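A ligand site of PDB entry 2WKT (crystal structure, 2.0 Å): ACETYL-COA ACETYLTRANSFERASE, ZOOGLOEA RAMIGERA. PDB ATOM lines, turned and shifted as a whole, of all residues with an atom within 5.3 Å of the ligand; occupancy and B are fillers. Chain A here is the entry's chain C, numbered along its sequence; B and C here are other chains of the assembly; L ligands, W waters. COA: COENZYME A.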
ATOM      1  N   CYS A  89       8.406 -13.600  29.207  1.00  0.00           N
ATOM      2  CA  CYS A  89       7.997 -14.964  28.889  1.00  0.00           C
ATOM      3  C   CYS A  89       6.829 -15.453  29.771  1.00  0.00           C
ATOM      4  O   CYS A  89       6.167 -16.437  29.430  1.00  0.00           O
ATOM      5  CB  CYS A  89       9.200 -15.915  29.003  1.00  0.00           C
ATOM      6  SG  CYS A  89      10.745 -15.288  28.205  1.00  0.00           S
ATOM      7  N   LEU A 148      14.740 -10.566  23.913  1.00  0.00           N
ATOM      8  CA  LEU A 148      15.633 -11.717  24.060  1.00  0.00           C
ATOM      9  C   LEU A 148      17.011 -11.433  24.658  1.00  0.00           C
ATOM     10  O   LEU A 148      17.878 -12.310  24.660  1.00  0.00           O
ATOM     11  CB  LEU A 148      15.785 -12.401  22.706  1.00  0.00           C
ATOM     12  CG  LEU A 148      14.489 -12.978  22.149  1.00  0.00           C
ATOM     13  CD1 LEU A 148      14.712 -13.494  20.752  1.00  0.00           C
ATOM     14  CD2 LEU A 148      14.013 -14.092  23.043  1.00  0.00           C
ATOM     15  N   HIS A 156      22.389 -12.874  25.430  1.00  0.00           N
ATOM     16  CA  HIS A 156      21.149 -13.510  25.021  1.00  0.00           C
ATOM     17  C   HIS A 156      20.646 -14.430  26.133  1.00  0.00           C
ATOM     18  O   HIS A 156      21.409 -14.863  27.000  1.00  0.00           O
ATOM     19  CB  HIS A 156      21.368 -14.273  23.717  1.00  0.00           C
ATOM     20  CG  HIS A 156      20.111 -14.716  23.036  1.00  0.00           C
ATOM     21  ND1 HIS A 156      19.475 -15.907  23.315  1.00  0.00           N
ATOM     22  CD2 HIS A 156      19.373 -14.122  22.055  1.00  0.00           C
ATOM     23  CE1 HIS A 156      18.398 -16.026  22.571  1.00  0.00           C
ATOM     24  NE2 HIS A 156      18.310 -14.960  21.787  1.00  0.00           N
ATOM     25  N   MET A 157      19.347 -14.699  26.140  1.00  0.00           N
ATOM     26  CA  MET A 157      18.791 -15.691  27.072  1.00  0.00           C
ATOM     27  C   MET A 157      19.553 -17.021  26.920  1.00  0.00           C
ATOM     28  O   MET A 157      19.744 -17.772  27.883  1.00  0.00           O
ATOM     29  CB  MET A 157      17.305 -15.897  26.819  1.00  0.00           C
ATOM     30  CG  MET A 157      16.407 -14.675  27.084  1.00  0.00           C
ATOM     31  SD  MET A 157      16.392 -14.086  28.793  1.00  0.00           S
ATOM     32  CE  MET A 157      17.643 -12.805  28.697  1.00  0.00           C
ATOM     33  N   GLY A 158      19.975 -17.308  25.683  1.00  0.00           N
ATOM     34  CA  GLY A 158      20.757 -18.498  25.395  1.00  0.00           C
ATOM     35  C   GLY A 158      22.006 -18.611  26.246  1.00  0.00           C
ATOM     36  O   GLY A 158      22.456 -19.707  26.550  1.00  0.00           O
ATOM     37  N   GLN A 183      10.286 -33.182  20.835  1.00  0.00           N
ATOM     38  CA  GLN A 183       9.834 -33.300  19.452  1.00  0.00           C
ATOM     39  C   GLN A 183       8.972 -34.546  19.252  1.00  0.00           C
ATOM     40  O   GLN A 183       7.888 -34.480  18.651  1.00  0.00           O
ATOM     41  CB  GLN A 183      11.017 -33.382  18.492  1.00  0.00           C
ATOM     42  CG  GLN A 183      11.903 -32.151  18.444  1.00  0.00           C
ATOM     43  CD  GLN A 183      11.303 -31.043  17.606  1.00  0.00           C
ATOM     44  OE1 GLN A 183      10.181 -31.151  17.106  1.00  0.00           O
ATOM     45  NE2 GLN A 183      12.062 -29.961  17.431  1.00  0.00           N
ATOM     46  N   TYR A 218       5.903 -25.793  13.506  1.00  0.00           N
ATOM     47  CA  TYR A 218       7.287 -25.745  13.958  1.00  0.00           C
ATOM     48  C   TYR A 218       7.801 -27.125  14.393  1.00  0.00           C
ATOM     49  O   TYR A 218       9.003 -27.351  14.523  1.00  0.00           O
ATOM     50  CB  TYR A 218       7.407 -24.731  15.090  1.00  0.00           C
ATOM     51  CG  TYR A 218       8.809 -24.514  15.573  1.00  0.00           C
ATOM     52  CD1 TYR A 218       9.794 -24.015  14.730  1.00  0.00           C
ATOM     53  CD2 TYR A 218       9.152 -24.784  16.891  1.00  0.00           C
ATOM     54  CE1 TYR A 218      11.097 -23.812  15.180  1.00  0.00           C
ATOM     55  CE2 TYR A 218      10.422 -24.591  17.353  1.00  0.00           C
ATOM     56  CZ  TYR A 218      11.401 -24.103  16.490  1.00  0.00           C
ATOM     57  OH  TYR A 218      12.681 -23.908  16.972  1.00  0.00           O
ATOM     58  N   ARG A 220       9.170 -30.659  14.360  1.00  0.00           N
ATOM     59  CA  ARG A 220       9.853 -31.499  13.390  1.00  0.00           C
ATOM     60  C   ARG A 220       9.489 -32.973  13.571  1.00  0.00           C
ATOM     61  O   ARG A 220       9.508 -33.502  14.685  1.00  0.00           O
ATOM     62  CB  ARG A 220      11.368 -31.273  13.359  1.00  0.00           C
ATOM     63  CG  ARG A 220      11.968 -30.743  14.630  1.00  0.00           C
ATOM     64  CD  ARG A 220      13.097 -29.768  14.308  1.00  0.00           C
ATOM     65  NE  ARG A 220      13.925 -30.248  13.210  1.00  0.00           N
ATOM     66  CZ  ARG A 220      14.513 -29.456  12.309  1.00  0.00           C
ATOM     67  NH1 ARG A 220      14.350 -28.143  12.357  1.00  0.00           N
ATOM     68  NH2 ARG A 220      15.247 -29.981  11.333  1.00  0.00           N
ATOM     69  N   ALA A 223      12.360 -36.526  14.600  1.00  0.00           N
ATOM     70  CA  ALA A 223      13.580 -36.006  15.225  1.00  0.00           C
ATOM     71  C   ALA A 223      14.408 -37.129  15.843  1.00  0.00           C
ATOM     72  O   ALA A 223      13.874 -38.011  16.510  1.00  0.00           O
ATOM     73  CB  ALA A 223      13.229 -34.957  16.267  1.00  0.00           C
ATOM     74  N   SER A 227      20.533 -36.393  14.353  1.00  0.00           N
ATOM     75  CA  SER A 227      20.424 -35.030  13.820  1.00  0.00           C
ATOM     76  C   SER A 227      20.695 -33.980  14.891  1.00  0.00           C
ATOM     77  O   SER A 227      21.356 -32.971  14.630  1.00  0.00           O
ATOM     78  CB  SER A 227      19.052 -34.798  13.152  1.00  0.00           C
ATOM     79  OG  SER A 227      18.001 -34.803  14.093  1.00  0.00           O
ATOM     80  N   MET A 228      20.196 -34.222  16.110  1.00  0.00           N
ATOM     81  CA  MET A 228      20.434 -33.310  17.233  1.00  0.00           C
ATOM     82  C   MET A 228      21.928 -33.082  17.485  1.00  0.00           C
ATOM     83  O   MET A 228      22.362 -31.958  17.769  1.00  0.00           O
ATOM     84  CB  MET A 228      19.757 -33.873  18.494  1.00  0.00           C
ATOM     85  CG  MET A 228      19.343 -32.807  19.497  1.00  0.00           C
ATOM     86  SD  MET A 228      18.067 -31.707  18.825  1.00  0.00           S
ATOM     87  CE  MET A 228      16.825 -32.909  18.340  1.00  0.00           C
ATOM     88  N   LEU A 231      24.270 -30.601  15.266  1.00  0.00           N
ATOM     89  CA  LEU A 231      24.103 -29.159  15.384  1.00  0.00           C
ATOM     90  C   LEU A 231      25.252 -28.492  16.148  1.00  0.00           C
ATOM     91  O   LEU A 231      25.844 -29.098  17.039  1.00  0.00           O
ATOM     92  CB  LEU A 231      22.770 -28.824  16.048  1.00  0.00           C
ATOM     93  CG  LEU A 231      21.568 -29.515  15.414  1.00  0.00           C
ATOM     94  CD1 LEU A 231      20.274 -29.153  16.136  1.00  0.00           C
ATOM     95  CD2 LEU A 231      21.477 -29.184  13.926  1.00  0.00           C
ATOM     96  N   ALA A 234      24.799 -22.622  19.608  1.00  0.00           N
ATOM     97  CA  ALA A 234      24.151 -21.417  19.097  1.00  0.00           C
ATOM     98  C   ALA A 234      24.658 -20.089  19.684  1.00  0.00           C
ATOM     99  O   ALA A 234      24.598 -19.055  19.010  1.00  0.00           O
ATOM    100  CB  ALA A 234      22.633 -21.529  19.269  1.00  0.00           C
ATOM    101  N   PHE A 235      25.166 -20.121  20.916  1.00  0.00           N
ATOM    102  CA  PHE A 235      25.569 -18.904  21.625  1.00  0.00           C
ATOM    103  C   PHE A 235      27.011 -18.896  22.131  1.00  0.00           C
ATOM    104  O   PHE A 235      27.641 -17.848  22.207  1.00  0.00           O
ATOM    105  CB  PHE A 235      24.634 -18.627  22.807  1.00  0.00           C
ATOM    106  CG  PHE A 235      23.186 -18.741  22.443  1.00  0.00           C
ATOM    107  CD1 PHE A 235      22.528 -17.678  21.851  1.00  0.00           C
ATOM    108  CD2 PHE A 235      22.479 -19.907  22.692  1.00  0.00           C
ATOM    109  CE1 PHE A 235      21.197 -17.772  21.509  1.00  0.00           C
ATOM    110  CE2 PHE A 235      21.151 -20.012  22.350  1.00  0.00           C
ATOM    111  CZ  PHE A 235      20.506 -18.945  21.756  1.00  0.00           C
ATOM    112  N   THR A 242      22.185 -25.309  21.537  1.00  0.00           N
ATOM    113  CA  THR A 242      22.089 -25.201  20.085  1.00  0.00           C
ATOM    114  C   THR A 242      20.667 -24.808  19.711  1.00  0.00           C
ATOM    115  O   THR A 242      19.779 -24.752  20.569  1.00  0.00           O
ATOM    116  CB  THR A 242      22.390 -26.551  19.402  1.00  0.00           C
ATOM    117  OG1 THR A 242      21.339 -27.482  19.689  1.00  0.00           O
ATOM    118  CG2 THR A 242      23.707 -27.115  19.882  1.00  0.00           C
ATOM    119  N   ALA A 243      20.443 -24.549  18.422  1.00  0.00           N
ATOM    120  CA  ALA A 243      19.105 -24.269  17.915  1.00  0.00           C
ATOM    121  C   ALA A 243      18.192 -25.471  18.163  1.00  0.00           C
ATOM    122  O   ALA A 243      16.967 -25.322  18.257  1.00  0.00           O
ATOM    123  CB  ALA A 243      19.148 -23.943  16.418  1.00  0.00           C
ATOM    124  N   GLY A 244      18.794 -26.649  18.302  1.00  0.00           N
ATOM    125  CA  GLY A 244      18.067 -27.895  18.430  1.00  0.00           C
ATOM    126  C   GLY A 244      17.510 -28.206  19.815  1.00  0.00           C
ATOM    127  O   GLY A 244      16.397 -28.724  19.933  1.00  0.00           O
ATOM    128  N   ALA A 246      17.108 -25.780  22.065  1.00  0.00           N
ATOM    129  CA  ALA A 246      16.572 -24.496  22.522  1.00  0.00           C
ATOM    130  C   ALA A 246      15.194 -24.260  21.912  1.00  0.00           C
ATOM    131  O   ALA A 246      14.889 -24.777  20.835  1.00  0.00           O
ATOM    132  CB  ALA A 246      17.506 -23.383  22.152  1.00  0.00           C
ATOM    133  N   SER A 247      14.364 -23.467  22.583  1.00  0.00           N
ATOM    134  CA  SER A 247      13.048 -23.148  22.051  1.00  0.00           C
ATOM    135  C   SER A 247      13.220 -22.305  20.778  1.00  0.00           C
ATOM    136  O   SER A 247      14.315 -21.878  20.438  1.00  0.00           O
ATOM    137  CB  SER A 247      12.189 -22.424  23.105  1.00  0.00           C
ATOM    138  OG  SER A 247      12.785 -21.206  23.537  1.00  0.00           O
ATOM    139  N   GLY A 248      12.123 -22.078  20.062  1.00  0.00           N
ATOM    140  CA  GLY A 248      12.205 -21.316  18.831  1.00  0.00           C
ATOM    141  C   GLY A 248      11.640 -19.909  18.951  1.00  0.00           C
ATOM    142  O   GLY A 248      11.101 -19.534  19.996  1.00  0.00           O
ATOM    143  N   LEU A 249      11.801 -19.127  17.879  1.00  0.00           N
ATOM    144  CA  LEU A 249      11.133 -17.843  17.748  1.00  0.00           C
ATOM    145  C   LEU A 249       9.849 -18.110  16.984  1.00  0.00           C
ATOM    146  O   LEU A 249       9.885 -18.777  15.951  1.00  0.00           O
ATOM    147  CB  LEU A 249      12.012 -16.866  16.946  1.00  0.00           C
ATOM    148  CG  LEU A 249      13.497 -16.774  17.317  1.00  0.00           C
ATOM    149  CD1 LEU A 249      14.295 -16.077  16.212  1.00  0.00           C
ATOM    150  CD2 LEU A 249      13.688 -16.070  18.664  1.00  0.00           C
ATOM    151  N   MET A 288      18.203 -17.012  34.992  1.00  0.00           N
ATOM    152  CA  MET A 288      16.760 -16.755  34.940  1.00  0.00           C
ATOM    153  C   MET A 288      15.950 -18.032  34.780  1.00  0.00           C
ATOM    154  O   MET A 288      14.790 -18.096  35.172  1.00  0.00           O
ATOM    155  CB  MET A 288      16.448 -15.793  33.790  1.00  0.00           C
ATOM    156  CG  MET A 288      16.644 -16.390  32.402  1.00  0.00           C
ATOM    157  SD  MET A 288      15.168 -17.180  31.690  1.00  0.00           S
ATOM    158  CE  MET A 288      15.838 -17.567  30.062  1.00  0.00           C
ATOM    159  N   ALA A 318      11.891 -23.215  27.654  1.00  0.00           N
ATOM    160  CA  ALA A 318      12.691 -22.134  27.098  1.00  0.00           C
ATOM    161  C   ALA A 318      13.996 -22.715  26.561  1.00  0.00           C
ATOM    162  O   ALA A 318      14.376 -22.451  25.427  1.00  0.00           O
ATOM    163  CB  ALA A 318      12.984 -21.089  28.158  1.00  0.00           C
ATOM    164  N   PHE A 319      14.674 -23.501  27.388  1.00  0.00           N
ATOM    165  CA  PHE A 319      15.858 -24.236  26.938  1.00  0.00           C
ATOM    166  C   PHE A 319      15.868 -25.613  27.575  1.00  0.00           C
ATOM    167  O   PHE A 319      15.390 -25.799  28.699  1.00  0.00           O
ATOM    168  CB  PHE A 319      17.144 -23.455  27.244  1.00  0.00           C
ATOM    169  CG  PHE A 319      17.200 -22.101  26.610  1.00  0.00           C
ATOM    170  CD1 PHE A 319      17.718 -21.934  25.335  1.00  0.00           C
ATOM    171  CD2 PHE A 319      16.694 -20.991  27.264  1.00  0.00           C
ATOM    172  CE1 PHE A 319      17.752 -20.693  24.730  1.00  0.00           C
ATOM    173  CE2 PHE A 319      16.711 -19.735  26.677  1.00  0.00           C
ATOM    174  CZ  PHE A 319      17.248 -19.583  25.398  1.00  0.00           C
ATOM    175  N   HIS A 348       7.670 -20.965  20.828  1.00  0.00           N
ATOM    176  CA  HIS A 348       7.624 -20.158  22.039  1.00  0.00           C
ATOM    177  C   HIS A 348       7.367 -18.685  21.707  1.00  0.00           C
ATOM    178  O   HIS A 348       8.302 -17.860  21.709  1.00  0.00           O
ATOM    179  CB  HIS A 348       8.939 -20.288  22.807  1.00  0.00           C
ATOM    180  CG  HIS A 348       8.903 -19.710  24.188  1.00  0.00           C
ATOM    181  ND1 HIS A 348       9.177 -18.378  24.442  1.00  0.00           N
ATOM    182  CD2 HIS A 348       8.658 -20.277  25.397  1.00  0.00           C
ATOM    183  CE1 HIS A 348       9.073 -18.155  25.745  1.00  0.00           C
ATOM    184  NE2 HIS A 348       8.771 -19.292  26.342  1.00  0.00           N
ATOM    185  N   ILE A 350       6.603 -15.468  22.702  1.00  0.00           N
ATOM    186  CA  ILE A 350       6.875 -14.971  24.050  1.00  0.00           C
ATOM    187  C   ILE A 350       5.651 -14.609  24.882  1.00  0.00           C
ATOM    188  O   ILE A 350       5.358 -15.286  25.880  1.00  0.00           O
ATOM    189  CB  ILE A 350       7.840 -13.784  24.043  1.00  0.00           C
ATOM    190  CG1 ILE A 350       9.080 -14.112  23.231  1.00  0.00           C
ATOM    191  CG2 ILE A 350       8.219 -13.409  25.469  1.00  0.00           C
ATOM    192  CD1 ILE A 350      10.161 -13.050  23.359  1.00  0.00           C
ATOM    193  N   CYS A 378       9.756 -19.822  32.918  1.00  0.00           N
ATOM    194  CA  CYS A 378      10.819 -18.926  33.374  1.00  0.00           C
ATOM    195  C   CYS A 378      10.638 -17.581  32.687  1.00  0.00           C
ATOM    196  O   CYS A 378       9.852 -17.440  31.764  1.00  0.00           O
ATOM    197  CB  CYS A 378      12.211 -19.517  33.129  1.00  0.00           C
ATOM    198  SG  CYS A 378      12.628 -19.808  31.390  1.00  0.00           S
ATOM    199  N   GLY A 380      12.786 -13.882  31.487  1.00  0.00           N
ATOM    200  CA  GLY A 380      14.038 -13.158  31.345  1.00  0.00           C
ATOM    201  C   GLY A 380      14.093 -11.994  32.335  1.00  0.00           C
ATOM    202  O   GLY A 380      13.059 -11.420  32.696  1.00  0.00           O
ATOM    203  N   LYS B 208      27.698 -22.676   1.979  1.00  0.00           N
ATOM    204  CA  LYS B 208      27.161 -24.009   1.756  1.00  0.00           C
ATOM    205  C   LYS B 208      27.086 -24.338   0.265  1.00  0.00           C
ATOM    206  O   LYS B 208      26.135 -24.975  -0.194  1.00  0.00           O
ATOM    207  CB  LYS B 208      25.797 -24.192   2.423  1.00  0.00           C
ATOM    208  CG  LYS B 208      25.863 -24.201   3.955  1.00  0.00           C
ATOM    209  CD  LYS B 208      24.590 -24.760   4.572  1.00  0.00           C
ATOM    210  CE  LYS B 208      24.717 -24.834   6.091  1.00  0.00           C
ATOM    211  NZ  LYS B 208      23.565 -25.549   6.726  1.00  0.00           N
ATOM    212  N   MET C 134      16.849 -11.347  11.358  1.00  0.00           N
ATOM    213  CA  MET C 134      17.041 -11.010  12.757  1.00  0.00           C
ATOM    214  C   MET C 134      18.421 -10.428  13.012  1.00  0.00           C
ATOM    215  O   MET C 134      19.371 -10.684  12.280  1.00  0.00           O
ATOM    216  CB  MET C 134      16.759 -12.218  13.671  1.00  0.00           C
ATOM    217  CG  MET C 134      17.895 -13.239  13.795  1.00  0.00           C
ATOM    218  SD  MET C 134      17.481 -14.526  14.995  1.00  0.00           S
ATOM    219  CE  MET C 134      19.085 -15.234  15.386  1.00  0.00           C
HETATM  220  N1A COA L   1      17.192 -31.362  13.790  1.00  0.00           N
HETATM  221  C2A COA L   1      17.824 -30.988  12.659  1.00  0.00           C
HETATM  222  N3A COA L   1      18.104 -29.659  12.445  1.00  0.00           N
HETATM  223  C4A COA L   1      17.747 -28.736  13.362  1.00  0.00           C
HETATM  224  C5A COA L   1      17.126 -29.106  14.476  1.00  0.00           C
HETATM  225  C6A COA L   1      16.843 -30.447  14.697  1.00  0.00           C
HETATM  226  N6A COA L   1      16.166 -30.851  15.914  1.00  0.00           N
HETATM  227  N7A COA L   1      16.891 -27.972  15.235  1.00  0.00           N
HETATM  228  C8A COA L   1      17.395 -26.855  14.523  1.00  0.00           C
HETATM  229  N9A COA L   1      17.927 -27.299  13.405  1.00  0.00           N
HETATM  230  C1B COA L   1      18.529 -26.482  12.359  1.00  0.00           C
HETATM  231  C2B COA L   1      18.010 -26.051  11.026  1.00  0.00           C
HETATM  232  O2B COA L   1      16.634 -25.838  10.846  1.00  0.00           O
HETATM  233  C3B COA L   1      18.973 -25.052  10.497  1.00  0.00           C
HETATM  234  O3B COA L   1      19.559 -25.285   9.262  1.00  0.00           O
HETATM  235  P3B COA L   1      19.621 -24.109   8.126  1.00  0.00           P
HETATM  236  O7A COA L   1      20.494 -24.675   6.838  1.00  0.00           O
HETATM  237  O8A COA L   1      20.353 -22.753   8.725  1.00  0.00           O
HETATM  238  O9A COA L   1      18.210 -23.792   7.690  1.00  0.00           O
HETATM  239  C4B COA L   1      19.767 -24.537  11.698  1.00  0.00           C
HETATM  240  O4B COA L   1      19.611 -25.568  12.783  1.00  0.00           O
HETATM  241  C5B COA L   1      19.722 -23.028  12.041  1.00  0.00           C
HETATM  242  O5B COA L   1      18.863 -22.595  13.093  1.00  0.00           O
HETATM  243  P1A COA L   1      17.274 -22.220  12.761  1.00  0.00           P
HETATM  244  O1A COA L   1      17.103 -21.820  11.174  1.00  0.00           O
HETATM  245  O2A COA L   1      16.384 -23.389  13.070  1.00  0.00           O
HETATM  246  O3A COA L   1      16.821 -20.920  13.699  1.00  0.00           O
HETATM  247  P2A COA L   1      17.865 -19.654  14.004  1.00  0.00           P
HETATM  248  O4A COA L   1      17.470 -18.448  13.171  1.00  0.00           O
HETATM  249  O5A COA L   1      19.440 -20.043  13.678  1.00  0.00           O
HETATM  250  O6A COA L   1      17.701 -19.262  15.596  1.00  0.00           O
HETATM  251  CBP COA L   1      18.160 -19.566  18.012  1.00  0.00           C
HETATM  252  CCP COA L   1      18.411 -20.007  16.555  1.00  0.00           C
HETATM  253  CDP COA L   1      19.102 -18.411  18.318  1.00  0.00           C
HETATM  254  CEP COA L   1      18.409 -20.737  18.966  1.00  0.00           C
HETATM  255  CAP COA L   1      16.704 -19.087  18.135  1.00  0.00           C
HETATM  256  OAP COA L   1      15.752 -20.030  17.730  1.00  0.00           O
HETATM  257  C9P COA L   1      16.385 -18.536  19.550  1.00  0.00           C
HETATM  258  O9P COA L   1      16.861 -17.524  19.945  1.00  0.00           O
HETATM  259  N8P COA L   1      15.654 -19.428  20.451  1.00  0.00           N
HETATM  260  C7P COA L   1      15.400 -19.024  21.835  1.00  0.00           C
HETATM  261  C6P COA L   1      14.417 -17.861  22.027  1.00  0.00           C
HETATM  262  C5P COA L   1      14.281 -17.388  23.473  1.00  0.00           C
HETATM  263  O5P COA L   1      15.235 -17.180  24.119  1.00  0.00           O
HETATM  264  N4P COA L   1      12.965 -17.144  24.038  1.00  0.00           N
HETATM  265  C3P COA L   1      12.890 -16.755  25.441  1.00  0.00           C
HETATM  266  C2P COA L   1      13.638 -17.630  26.455  1.00  0.00           C
HETATM  267  S1P COA L   1      13.043 -17.584  28.181  1.00  0.00           S
HETATM  268  O   HOH W   1      16.274 -34.014  15.686  1.00  0.00           O
HETATM  269  O   HOH W   2      15.939 -23.042  17.968  1.00  0.00           O
HETATM  270  O   HOH W   3      21.567 -20.222  16.005  1.00  0.00           O
HETATM  271  O   HOH W   4      14.804 -25.683  12.623  1.00  0.00           O
HETATM  272  O   HOH W   5      17.798 -14.920  18.718  1.00  0.00           O
HETATM  273  O   HOH W   6      10.929 -17.284  21.577  1.00  0.00           O
HETATM  274  O   HOH W   7      14.716 -29.468  18.052  1.00  0.00           O
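Water W4 bridges the guanidinium group of Arg 220 (2.5 Å) and an oxygen (O2B) of the ligand (2.6 Å).
Water W7 lies within hydrogen-bond range of O of Gly 244, NE2 of Gln 183 and N6A of the ligand.
Water W5 lies within hydrogen-bond range of O9P of the ligand (3.0 Å), NE2 of His 156 (3.1 Å) and SD of Met 134 of chain C (3.8 Å).
Water W2 lies within hydrogen-bond range of the backbone carbonyl oxygen (O) of Ala 243 (2.5 Å), an oxygen (OAP) of the ligand (3.0 Å) and the backbone carbonyl oxygen (O) of Ser 247 (3.2 Å).
Water W1 bridges the side-chain hydroxyl (OG) of Ser 227 (2.5 Å) and a nitrogen (N6A) of the ligand (3.2 Å).
Water W6 lies within hydrogen-bond range of O of His 348, O of Gly 248 and N4P of the ligand.
The backbone carbonyl oxygen (O) of Ala 318 lies within hydrogen-bond range of the side-chain hydroxyl (OG) of Ser 247, at 2.8 Å.
OE1 of Gln 183 sits at hydrogen-bond distance from N of Arg 220, at 3.0 Å.
O of Leu 148 is in hydrogen-bond range of N of Met 157 (3.2 Å).
SD of Met 288 sits at hydrogen-bond distance from SG of Cys 378.
A ring nitrogen (ND1) of His 156 lies within hydrogen-bond range of the backbone NH of Gly 158, at 2.8 Å.
The side-chain hydroxyl (OG1) of Thr 242 sits close to the backbone NH (N) of Gly 244, 3.0 Å away.
Leu 148 touches the ligand (CD2 to C5P, 3.3 Å).
Met 157 touches the ligand (CB to O5P, 3.6 Å).
OG of Ser 227 touches N1A of the ligand (3.5 Å).
CD1 of Leu 231 touches C5A of the ligand, 3.6 Å away.
Phe 235 touches the ligand.
CB of Ala 243 touches O5B of the ligand, 3.6 Å away.
Gly 244 touches the ligand.
Gly 248 touches the ligand (CA to OAP, 3.9 Å).
Leu 249 touches the ligand (CD2 to O9P, 3.7 Å).
Met 288 touches the ligand.
Ala 318 touches the ligand.
CZ of Phe 319 touches O5P of the ligand (3.4 Å).
Cys 378 touches the ligand.
Hydrophobic or aromatic side chains within 4 Å of the ligand: Leu 148, His 156, Met 157, Met 228, Leu 231, Phe 235, Ala 243, Leu 249, Met 288, Ala 318 and Phe 319.
The nearest printed residue that does not touch the ligand is His 348 (4.004 Å).
The backbone carbonyl oxygen (O) of Ser 247 sits at hydrogen-bond distance from a nitrogen (N8P) of the ligand (2.8 Å).
N3A of the ligand sits close to NH2 of Arg 220 (3.1 Å).
The side-chain amino group (NZ) of Lys 208 of chain B lies within salt-bridge range of an oxygen (O7A) of the ligand, at 3.2 Å.
SG of Cys 89 sits close to S1P of the ligand.
The side-chain sulfur of Met 228 lies close to a nitrogen (N6A) of the ligand (3.6 Å).
A ring nitrogen (NE2) of His 156 sits close to an oxygen (O9P) of the ligand.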
